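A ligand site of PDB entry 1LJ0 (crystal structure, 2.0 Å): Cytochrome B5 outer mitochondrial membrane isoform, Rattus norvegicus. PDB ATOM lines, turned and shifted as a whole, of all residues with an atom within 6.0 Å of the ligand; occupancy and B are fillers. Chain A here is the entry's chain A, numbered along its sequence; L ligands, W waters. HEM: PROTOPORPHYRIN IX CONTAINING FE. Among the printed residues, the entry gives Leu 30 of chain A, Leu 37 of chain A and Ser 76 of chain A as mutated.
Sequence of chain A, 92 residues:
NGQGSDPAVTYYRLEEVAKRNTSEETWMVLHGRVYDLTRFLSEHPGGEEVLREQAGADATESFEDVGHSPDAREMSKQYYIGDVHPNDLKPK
A ring nitrogen (NE2) of His 68 is bound to an iron atom (FE) of the ligand (2.1 Å). An oxygen (O2A) of the ligand lies within hydrogen-bond range of the side-chain hydroxyl of Ser 69, 2.6 Å away. An iron atom (FE) of the ligand is bound by a ring nitrogen (NE2) of His 44, 2.2 Å away. The backbone NH (N) of Ser 69 lies within hydrogen-bond range of an oxygen (O1A) of the ligand (2.8 Å).
OG of Ser 69 lies close to N of Asp 71 (3.2 Å). N of Gly 46 sits close to ND1 of His 44 (3.4 Å). ND1 of His 68 is in hydrogen-bond range of O of Phe 63, 2.7 Å away. The backbone carbonyl oxygen of Met 28 sits at hydrogen-bond distance from the backbone NH of Tyr 35. The side-chain hydroxyl (OG) of Ser 76 lies within hydrogen-bond range of the backbone carbonyl oxygen (O) of Arg 73. OG of Ser 69 is in hydrogen-bond range of N of Ala 72, at 3.0 Å. The side-chain amide nitrogen (NE2) of Gln 54 lies within hydrogen-bond range of the side-chain hydroxyl (OG) of Ser 62.
Residues that only touch the ligand: Val 50 (3.3 Å), Leu 37 (3.3 Å), Gln 54 (3.4 Å), Phe 40 (3.4 Å), Phe 63 (3.4 Å), Pro 45 (3.5 Å), Met 28 (3.5 Å), Ser 76 (3.6 Å), Ala 72 (3.6 Å), Val 66 (3.6 Å), Leu 51 (3.6 Å), Gly 46 (3.7 Å), Leu 30 (3.7 Å), Ala 59 (3.7 Å), Ser 62 (3.8 Å) and Met 75 (3.8 Å).
Water W1 lies within hydrogen-bond range of O of Val 50 (2.8 Å), OE1 of Glu 53 (2.8 Å) and NE2 of Gln 54 (3.2 Å).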
ATOM      1  N   MET A  28     -16.932   5.022  -9.134  1.00  0.00           N
ATOM      2  CA  MET A  28     -16.682   6.144  -8.262  1.00  0.00           C
ATOM      3  C   MET A  28     -17.650   6.042  -7.058  1.00  0.00           C
ATOM      4  O   MET A  28     -18.764   5.532  -7.177  1.00  0.00           O
ATOM      5  CB  MET A  28     -16.891   7.440  -9.057  1.00  0.00           C
ATOM      6  CG  MET A  28     -16.710   8.672  -8.264  1.00  0.00           C
ATOM      7  SD  MET A  28     -16.747  10.104  -9.307  1.00  0.00           S
ATOM      8  CE  MET A  28     -15.267   9.849 -10.330  1.00  0.00           C
ATOM      9  N   LEU A  30     -20.112   7.880  -4.199  1.00  0.00           N
ATOM     10  CA  LEU A  30     -20.800   9.143  -3.822  1.00  0.00           C
ATOM     11  C   LEU A  30     -21.727   8.789  -2.656  1.00  0.00           C
ATOM     12  O   LEU A  30     -22.556   7.904  -2.782  1.00  0.00           O
ATOM     13  CB  LEU A  30     -21.635   9.722  -4.980  1.00  0.00           C
ATOM     14  CG  LEU A  30     -20.884  10.121  -6.274  1.00  0.00           C
ATOM     15  CD1 LEU A  30     -21.938  10.460  -7.372  1.00  0.00           C
ATOM     16  CD2 LEU A  30     -19.926  11.288  -6.019  1.00  0.00           C
ATOM     17  N   TYR A  35     -20.940   3.808  -8.179  1.00  0.00           N
ATOM     18  CA  TYR A  35     -21.518   4.121  -9.463  1.00  0.00           C
ATOM     19  C   TYR A  35     -20.587   3.710 -10.558  1.00  0.00           C
ATOM     20  O   TYR A  35     -19.390   3.968 -10.451  1.00  0.00           O
ATOM     21  CB  TYR A  35     -21.754   5.604  -9.610  1.00  0.00           C
ATOM     22  CG  TYR A  35     -22.800   6.114  -8.682  1.00  0.00           C
ATOM     23  CD1 TYR A  35     -22.485   6.427  -7.340  1.00  0.00           C
ATOM     24  CD2 TYR A  35     -24.139   6.192  -9.083  1.00  0.00           C
ATOM     25  CE1 TYR A  35     -23.461   6.771  -6.431  1.00  0.00           C
ATOM     26  CE2 TYR A  35     -25.142   6.549  -8.187  1.00  0.00           C
ATOM     27  CZ  TYR A  35     -24.807   6.826  -6.853  1.00  0.00           C
ATOM     28  OH  TYR A  35     -25.780   7.146  -5.943  1.00  0.00           O
ATOM     29  N   LEU A  37     -19.469   4.636 -13.803  1.00  0.00           N
ATOM     30  CA  LEU A  37     -19.532   5.740 -14.742  1.00  0.00           C
ATOM     31  C   LEU A  37     -18.864   5.494 -16.101  1.00  0.00           C
ATOM     32  O   LEU A  37     -18.775   6.423 -16.922  1.00  0.00           O
ATOM     33  CB  LEU A  37     -18.895   6.982 -14.104  1.00  0.00           C
ATOM     34  CG  LEU A  37     -19.513   7.376 -12.749  1.00  0.00           C
ATOM     35  CD1 LEU A  37     -18.783   8.612 -12.193  1.00  0.00           C
ATOM     36  CD2 LEU A  37     -21.037   7.619 -12.906  1.00  0.00           C
ATOM     37  N   PHE A  40     -20.684   6.869 -18.694  1.00  0.00           N
ATOM     38  CA  PHE A  40     -21.028   8.243 -18.424  1.00  0.00           C
ATOM     39  C   PHE A  40     -19.940   9.275 -18.727  1.00  0.00           C
ATOM     40  O   PHE A  40     -20.255  10.434 -18.943  1.00  0.00           O
ATOM     41  CB  PHE A  40     -21.451   8.432 -16.977  1.00  0.00           C
ATOM     42  CG  PHE A  40     -21.834   9.849 -16.655  1.00  0.00           C
ATOM     43  CD1 PHE A  40     -22.914  10.473 -17.291  1.00  0.00           C
ATOM     44  CD2 PHE A  40     -21.109  10.566 -15.729  1.00  0.00           C
ATOM     45  CE1 PHE A  40     -23.265  11.797 -17.006  1.00  0.00           C
ATOM     46  CE2 PHE A  40     -21.441  11.913 -15.437  1.00  0.00           C
ATOM     47  CZ  PHE A  40     -22.531  12.511 -16.081  1.00  0.00           C
ATOM     48  N   HIS A  44     -20.476  13.678 -19.549  1.00  0.00           N
ATOM     49  CA  HIS A  44     -20.377  14.507 -18.375  1.00  0.00           C
ATOM     50  C   HIS A  44     -20.071  15.941 -18.731  1.00  0.00           C
ATOM     51  O   HIS A  44     -18.980  16.240 -19.182  1.00  0.00           O
ATOM     52  CB  HIS A  44     -19.255  14.001 -17.466  1.00  0.00           C
ATOM     53  CG  HIS A  44     -19.086  14.818 -16.230  1.00  0.00           C
ATOM     54  ND1 HIS A  44     -17.884  15.363 -15.849  1.00  0.00           N
ATOM     55  CD2 HIS A  44     -19.966  15.132 -15.254  1.00  0.00           C
ATOM     56  CE1 HIS A  44     -18.029  15.973 -14.679  1.00  0.00           C
ATOM     57  NE2 HIS A  44     -19.284  15.845 -14.297  1.00  0.00           N
ATOM     58  N   PRO A  45     -21.007  16.850 -18.447  1.00  0.00           N
ATOM     59  CA  PRO A  45     -20.842  18.272 -18.737  1.00  0.00           C
ATOM     60  C   PRO A  45     -19.559  18.868 -18.157  1.00  0.00           C
ATOM     61  O   PRO A  45     -19.021  19.808 -18.735  1.00  0.00           O
ATOM     62  CB  PRO A  45     -22.104  18.868 -18.143  1.00  0.00           C
ATOM     63  CG  PRO A  45     -23.134  17.769 -18.363  1.00  0.00           C
ATOM     64  CD  PRO A  45     -22.341  16.581 -17.876  1.00  0.00           C
ATOM     65  N   GLY A  46     -19.054  18.343 -17.036  1.00  0.00           N
ATOM     66  CA  GLY A  46     -17.815  18.903 -16.522  1.00  0.00           C
ATOM     67  C   GLY A  46     -16.549  18.287 -17.128  1.00  0.00           C
ATOM     68  O   GLY A  46     -15.422  18.581 -16.685  1.00  0.00           O
ATOM     69  N   VAL A  50     -11.887  15.649 -14.822  1.00  0.00           N
ATOM     70  CA  VAL A  50     -12.247  15.745 -13.396  1.00  0.00           C
ATOM     71  C   VAL A  50     -12.736  14.389 -12.844  1.00  0.00           C
ATOM     72  O   VAL A  50     -12.588  14.148 -11.667  1.00  0.00           O
ATOM     73  CB  VAL A  50     -13.346  16.823 -13.101  1.00  0.00           C
ATOM     74  CG1 VAL A  50     -12.830  18.194 -13.485  1.00  0.00           C
ATOM     75  CG2 VAL A  50     -14.635  16.493 -13.850  1.00  0.00           C
ATOM     76  N   LEU A  51     -13.309  13.525 -13.686  1.00  0.00           N
ATOM     77  CA  LEU A  51     -13.766  12.203 -13.224  1.00  0.00           C
ATOM     78  C   LEU A  51     -12.561  11.275 -13.172  1.00  0.00           C
ATOM     79  O   LEU A  51     -12.391  10.514 -12.199  1.00  0.00           O
ATOM     80  CB  LEU A  51     -14.855  11.628 -14.156  1.00  0.00           C
ATOM     81  CG  LEU A  51     -16.141  12.477 -14.268  1.00  0.00           C
ATOM     82  CD1 LEU A  51     -17.211  11.770 -15.170  1.00  0.00           C
ATOM     83  CD2 LEU A  51     -16.689  12.703 -12.852  1.00  0.00           C
ATOM     84  N   GLU A  53      -9.635  12.008 -12.560  1.00  0.00           N
ATOM     85  CA  GLU A  53      -8.831  12.334 -11.370  1.00  0.00           C
ATOM     86  C   GLU A  53      -9.241  11.600 -10.103  1.00  0.00           C
ATOM     87  O   GLU A  53      -8.411  11.262  -9.283  1.00  0.00           O
ATOM     88  CB  GLU A  53      -8.869  13.832 -11.060  1.00  0.00           C
ATOM     89  CG  GLU A  53      -8.492  14.742 -12.206  1.00  0.00           C
ATOM     90  CD  GLU A  53      -8.321  16.201 -11.777  1.00  0.00           C
ATOM     91  OE1 GLU A  53      -9.020  16.675 -10.836  1.00  0.00           O
ATOM     92  OE2 GLU A  53      -7.489  16.889 -12.415  1.00  0.00           O
ATOM     93  N   GLN A  54     -10.538  11.386  -9.919  1.00  0.00           N
ATOM     94  CA  GLN A  54     -10.938  10.684  -8.715  1.00  0.00           C
ATOM     95  C   GLN A  54     -11.548   9.331  -9.006  1.00  0.00           C
ATOM     96  O   GLN A  54     -12.279   8.781  -8.195  1.00  0.00           O
ATOM     97  CB  GLN A  54     -11.906  11.551  -7.915  1.00  0.00           C
ATOM     98  CG  GLN A  54     -11.223  12.806  -7.417  1.00  0.00           C
ATOM     99  CD  GLN A  54     -12.104  13.614  -6.522  1.00  0.00           C
ATOM    100  OE1 GLN A  54     -12.475  13.186  -5.452  1.00  0.00           O
ATOM    101  NE2 GLN A  54     -12.432  14.801  -6.967  1.00  0.00           N
ATOM    102  N   ALA A  59     -15.736  10.377  -4.329  1.00  0.00           N
ATOM    103  CA  ALA A  59     -15.636  11.768  -4.796  1.00  0.00           C
ATOM    104  C   ALA A  59     -16.829  12.630  -4.305  1.00  0.00           C
ATOM    105  O   ALA A  59     -17.150  13.684  -4.854  1.00  0.00           O
ATOM    106  CB  ALA A  59     -15.483  11.811  -6.312  1.00  0.00           C
ATOM    107  N   SER A  62     -15.923  16.558  -3.723  1.00  0.00           N
ATOM    108  CA  SER A  62     -15.825  17.337  -4.946  1.00  0.00           C
ATOM    109  C   SER A  62     -17.176  17.413  -5.651  1.00  0.00           C
ATOM    110  O   SER A  62     -17.501  18.428  -6.271  1.00  0.00           O
ATOM    111  CB  SER A  62     -14.781  16.728  -5.903  1.00  0.00           C
ATOM    112  OG  SER A  62     -13.505  16.617  -5.303  1.00  0.00           O
ATOM    113  N   PHE A  63     -17.962  16.345  -5.590  1.00  0.00           N
ATOM    114  CA  PHE A  63     -19.291  16.330  -6.230  1.00  0.00           C
ATOM    115  C   PHE A  63     -20.183  17.392  -5.611  1.00  0.00           C
ATOM    116  O   PHE A  63     -20.866  18.129  -6.320  1.00  0.00           O
ATOM    117  CB  PHE A  63     -19.951  14.976  -6.068  1.00  0.00           C
ATOM    118  CG  PHE A  63     -21.307  14.882  -6.674  1.00  0.00           C
ATOM    119  CD1 PHE A  63     -21.445  14.626  -8.065  1.00  0.00           C
ATOM    120  CD2 PHE A  63     -22.443  15.035  -5.900  1.00  0.00           C
ATOM    121  CE1 PHE A  63     -22.677  14.524  -8.633  1.00  0.00           C
ATOM    122  CE2 PHE A  63     -23.742  14.922  -6.484  1.00  0.00           C
ATOM    123  CZ  PHE A  63     -23.852  14.657  -7.853  1.00  0.00           C
ATOM    124  N   VAL A  66     -18.895  21.157  -6.095  1.00  0.00           N
ATOM    125  CA  VAL A  66     -19.178  21.685  -7.417  1.00  0.00           C
ATOM    126  C   VAL A  66     -20.633  22.221  -7.440  1.00  0.00           C
ATOM    127  O   VAL A  66     -20.959  23.142  -8.182  1.00  0.00           O
ATOM    128  CB  VAL A  66     -19.040  20.560  -8.527  1.00  0.00           C
ATOM    129  CG1 VAL A  66     -19.827  20.937  -9.738  1.00  0.00           C
ATOM    130  CG2 VAL A  66     -17.601  20.356  -8.898  1.00  0.00           C
ATOM    131  N   GLY A  67     -21.519  21.652  -6.626  1.00  0.00           N
ATOM    132  CA  GLY A  67     -22.898  22.131  -6.622  1.00  0.00           C
ATOM    133  C   GLY A  67     -23.805  21.565  -7.706  1.00  0.00           C
ATOM    134  O   GLY A  67     -24.558  22.313  -8.373  1.00  0.00           O
ATOM    135  N   HIS A  68     -23.821  20.246  -7.859  1.00  0.00           N
ATOM    136  CA  HIS A  68     -24.654  19.648  -8.893  1.00  0.00           C
ATOM    137  C   HIS A  68     -26.136  19.883  -8.724  1.00  0.00           C
ATOM    138  O   HIS A  68     -26.659  19.910  -7.598  1.00  0.00           O
ATOM    139  CB  HIS A  68     -24.383  18.148  -9.029  1.00  0.00           C
ATOM    140  CG  HIS A  68     -23.038  17.827  -9.596  1.00  0.00           C
ATOM    141  ND1 HIS A  68     -21.883  17.918  -8.861  1.00  0.00           N
ATOM    142  CD2 HIS A  68     -22.668  17.478 -10.849  1.00  0.00           C
ATOM    143  CE1 HIS A  68     -20.844  17.633  -9.630  1.00  0.00           C
ATOM    144  NE2 HIS A  68     -21.301  17.368 -10.846  1.00  0.00           N
ATOM    145  N   SER A  69     -26.808  20.010  -9.863  1.00  0.00           N
ATOM    146  CA  SER A  69     -28.228  20.246  -9.909  1.00  0.00           C
ATOM    147  C   SER A  69     -29.067  19.015  -9.596  1.00  0.00           C
ATOM    148  O   SER A  69     -28.564  17.885  -9.576  1.00  0.00           O
ATOM    149  CB  SER A  69     -28.612  20.696 -11.321  1.00  0.00           C
ATOM    150  OG  SER A  69     -28.629  19.574 -12.223  1.00  0.00           O
ATOM    151  N   PRO A  70     -30.367  19.225  -9.322  1.00  0.00           N
ATOM    152  CA  PRO A  70     -31.279  18.122  -9.038  1.00  0.00           C
ATOM    153  C   PRO A  70     -31.212  17.160 -10.241  1.00  0.00           C
ATOM    154  O   PRO A  70     -31.252  15.921 -10.102  1.00  0.00           O
ATOM    155  CB  PRO A  70     -32.651  18.808  -8.982  1.00  0.00           C
ATOM    156  CG  PRO A  70     -32.309  20.208  -8.576  1.00  0.00           C
ATOM    157  CD  PRO A  70     -31.005  20.544  -9.153  1.00  0.00           C
ATOM    158  N   ASP A  71     -31.100  17.728 -11.450  1.00  0.00           N
ATOM    159  CA  ASP A  71     -31.089  16.851 -12.642  1.00  0.00           C
ATOM    160  C   ASP A  71     -29.814  16.004 -12.722  1.00  0.00           C
ATOM    161  O   ASP A  71     -29.830  14.878 -13.191  1.00  0.00           O
ATOM    162  CB  ASP A  71     -31.329  17.629 -13.962  1.00  0.00           C
ATOM    163  CG  ASP A  71     -32.757  18.215 -14.050  1.00  0.00           C
ATOM    164  OD1 ASP A  71     -33.742  17.459 -13.874  1.00  0.00           O
ATOM    165  OD2 ASP A  71     -32.901  19.442 -14.276  1.00  0.00           O
ATOM    166  N   ALA A  72     -28.712  16.535 -12.214  1.00  0.00           N
ATOM    167  CA  ALA A  72     -27.444  15.821 -12.214  1.00  0.00           C
ATOM    168  C   ALA A  72     -27.581  14.654 -11.229  1.00  0.00           C
ATOM    169  O   ALA A  72     -27.176  13.519 -11.507  1.00  0.00           O
ATOM    170  CB  ALA A  72     -26.292  16.780 -11.831  1.00  0.00           C
ATOM    171  N   ARG A  73     -28.191  14.920 -10.095  1.00  0.00           N
ATOM    172  CA  ARG A  73     -28.409  13.859  -9.139  1.00  0.00           C
ATOM    173  C   ARG A  73     -29.324  12.761  -9.710  1.00  0.00           C
ATOM    174  O   ARG A  73     -29.061  11.576  -9.550  1.00  0.00           O
ATOM    175  CB  ARG A  73     -29.023  14.420  -7.848  1.00  0.00           C
ATOM    176  CG  ARG A  73     -28.082  15.343  -7.147  1.00  0.00           C
ATOM    177  CD  ARG A  73     -28.812  16.000  -5.986  1.00  0.00           C
ATOM    178  NE  ARG A  73     -28.086  17.165  -5.495  1.00  0.00           N
ATOM    179  CZ  ARG A  73     -27.031  17.147  -4.675  1.00  0.00           C
ATOM    180  NH1 ARG A  73     -26.528  16.007  -4.251  1.00  0.00           N
ATOM    181  NH2 ARG A  73     -26.521  18.298  -4.229  1.00  0.00           N
ATOM    182  N   MET A  75     -29.718  11.907 -12.739  1.00  0.00           N
ATOM    183  CA  MET A  75     -28.914  11.276 -13.790  1.00  0.00           C
ATOM    184  C   MET A  75     -27.938  10.222 -13.211  1.00  0.00           C
ATOM    185  O   MET A  75     -27.652   9.211 -13.826  1.00  0.00           O
ATOM    186  CB  MET A  75     -28.161  12.388 -14.528  1.00  0.00           C
ATOM    187  CG  MET A  75     -27.436  11.995 -15.776  1.00  0.00           C
ATOM    188  SD  MET A  75     -26.494  13.383 -16.552  1.00  0.00           S
ATOM    189  CE  MET A  75     -27.799  14.553 -16.995  1.00  0.00           C
ATOM    190  N   SER A  76     -27.457  10.436 -12.008  1.00  0.00           N
ATOM    191  CA  SER A  76     -26.531   9.480 -11.413  1.00  0.00           C
ATOM    192  C   SER A  76     -27.168   8.130 -11.086  1.00  0.00           C
ATOM    193  O   SER A  76     -26.482   7.103 -11.072  1.00  0.00           O
ATOM    194  CB  SER A  76     -25.963  10.040 -10.141  1.00  0.00           C
ATOM    195  OG  SER A  76     -26.949  10.013  -9.131  1.00  0.00           O
ATOM    196  N   TYR A  79     -26.527   4.768 -12.896  1.00  0.00           N
ATOM    197  CA  TYR A  79     -25.188   4.137 -12.814  1.00  0.00           C
ATOM    198  C   TYR A  79     -24.946   3.458 -11.465  1.00  0.00           C
ATOM    199  O   TYR A  79     -23.895   2.848 -11.263  1.00  0.00           O
ATOM    200  CB  TYR A  79     -24.135   5.221 -13.069  1.00  0.00           C
ATOM    201  CG  TYR A  79     -24.348   5.922 -14.424  1.00  0.00           C
ATOM    202  CD1 TYR A  79     -24.195   5.215 -15.614  1.00  0.00           C
ATOM    203  CD2 TYR A  79     -24.763   7.251 -14.505  1.00  0.00           C
ATOM    204  CE1 TYR A  79     -24.462   5.819 -16.875  1.00  0.00           C
ATOM    205  CE2 TYR A  79     -25.045   7.875 -15.762  1.00  0.00           C
ATOM    206  CZ  TYR A  79     -24.879   7.141 -16.929  1.00  0.00           C
ATOM    207  OH  TYR A  79     -25.138   7.706 -18.150  1.00  0.00           O
HETATM  208  CHA HEM L   1     -21.366  19.537 -14.228  1.00  0.00           C
HETATM  209  CHB HEM L   1     -23.371  15.217 -13.730  1.00  0.00           C
HETATM  210  CHC HEM L   1     -19.749  13.734 -10.917  1.00  0.00           C
HETATM  211  CHD HEM L   1     -17.561  17.975 -11.635  1.00  0.00           C
HETATM  212  C1A HEM L   1     -22.255  18.509 -14.304  1.00  0.00           C
HETATM  213  C2A HEM L   1     -23.515  18.604 -14.900  1.00  0.00           C
HETATM  214  C3A HEM L   1     -24.088  17.351 -14.827  1.00  0.00           C
HETATM  215  C4A HEM L   1     -23.161  16.522 -14.093  1.00  0.00           C
HETATM  216  CMA HEM L   1     -25.358  16.980 -15.342  1.00  0.00           C
HETATM  217  CAA HEM L   1     -24.145  19.870 -15.513  1.00  0.00           C
HETATM  218  CBA HEM L   1     -24.608  20.943 -14.454  1.00  0.00           C
HETATM  219  CGA HEM L   1     -25.584  20.383 -13.446  1.00  0.00           C
HETATM  220  O1A HEM L   1     -25.284  20.436 -12.231  1.00  0.00           O
HETATM  221  O2A HEM L   1     -26.593  19.784 -13.891  1.00  0.00           O
HETATM  222  C1B HEM L   1     -22.538  14.451 -12.942  1.00  0.00           C
HETATM  223  C2B HEM L   1     -22.854  13.078 -12.548  1.00  0.00           C
HETATM  224  C3B HEM L   1     -21.847  12.609 -11.705  1.00  0.00           C
HETATM  225  C4B HEM L   1     -20.909  13.753 -11.651  1.00  0.00           C
HETATM  226  CMB HEM L   1     -24.139  12.384 -13.008  1.00  0.00           C
HETATM  227  CAB HEM L   1     -21.695  11.273 -10.993  1.00  0.00           C
HETATM  228  CBB HEM L   1     -22.616  10.123 -11.365  1.00  0.00           C
HETATM  229  C1C HEM L   1     -18.861  14.758 -10.827  1.00  0.00           C
HETATM  230  C2C HEM L   1     -17.662  14.728 -10.027  1.00  0.00           C
HETATM  231  C3C HEM L   1     -16.993  15.893 -10.241  1.00  0.00           C
HETATM  232  C4C HEM L   1     -17.831  16.674 -11.172  1.00  0.00           C
HETATM  233  CMC HEM L   1     -17.249  13.595  -9.078  1.00  0.00           C
HETATM  234  CAC HEM L   1     -15.696  16.342  -9.635  1.00  0.00           C
HETATM  235  CBC HEM L   1     -14.606  15.567  -9.469  1.00  0.00           C
HETATM  236  C1D HEM L   1     -18.418  18.763 -12.418  1.00  0.00           C
HETATM  237  C2D HEM L   1     -18.142  20.140 -12.807  1.00  0.00           C
HETATM  238  C3D HEM L   1     -19.227  20.597 -13.528  1.00  0.00           C
HETATM  239  C4D HEM L   1     -20.138  19.473 -13.597  1.00  0.00           C
HETATM  240  CMD HEM L   1     -16.909  20.966 -12.462  1.00  0.00           C
HETATM  241  CAD HEM L   1     -19.444  22.021 -14.103  1.00  0.00           C
HETATM  242  CBD HEM L   1     -20.275  22.913 -13.158  1.00  0.00           C
HETATM  243  CGD HEM L   1     -21.202  23.898 -13.870  1.00  0.00           C
HETATM  244  O1D HEM L   1     -22.422  23.664 -13.906  1.00  0.00           O
HETATM  245  O2D HEM L   1     -20.725  25.026 -14.134  1.00  0.00           O
HETATM  246  NA  HEM L   1     -22.038  17.244 -13.765  1.00  0.00           N
HETATM  247  NB  HEM L   1     -21.339  14.861 -12.401  1.00  0.00           N
HETATM  248  NC  HEM L   1     -18.983  15.967 -11.513  1.00  0.00           N
HETATM  249  ND  HEM L   1     -19.641  18.344 -12.905  1.00  0.00           N
HETATM  250 FE   HEM L   1     -20.504  16.609 -12.671  1.00  0.00          FE
HETATM  251  O   HOH W   1     -11.525  15.939  -9.839  1.00  0.00           O
HETATM  252  O   HOH W   2     -27.643  19.998 -16.109  1.00  0.00           O
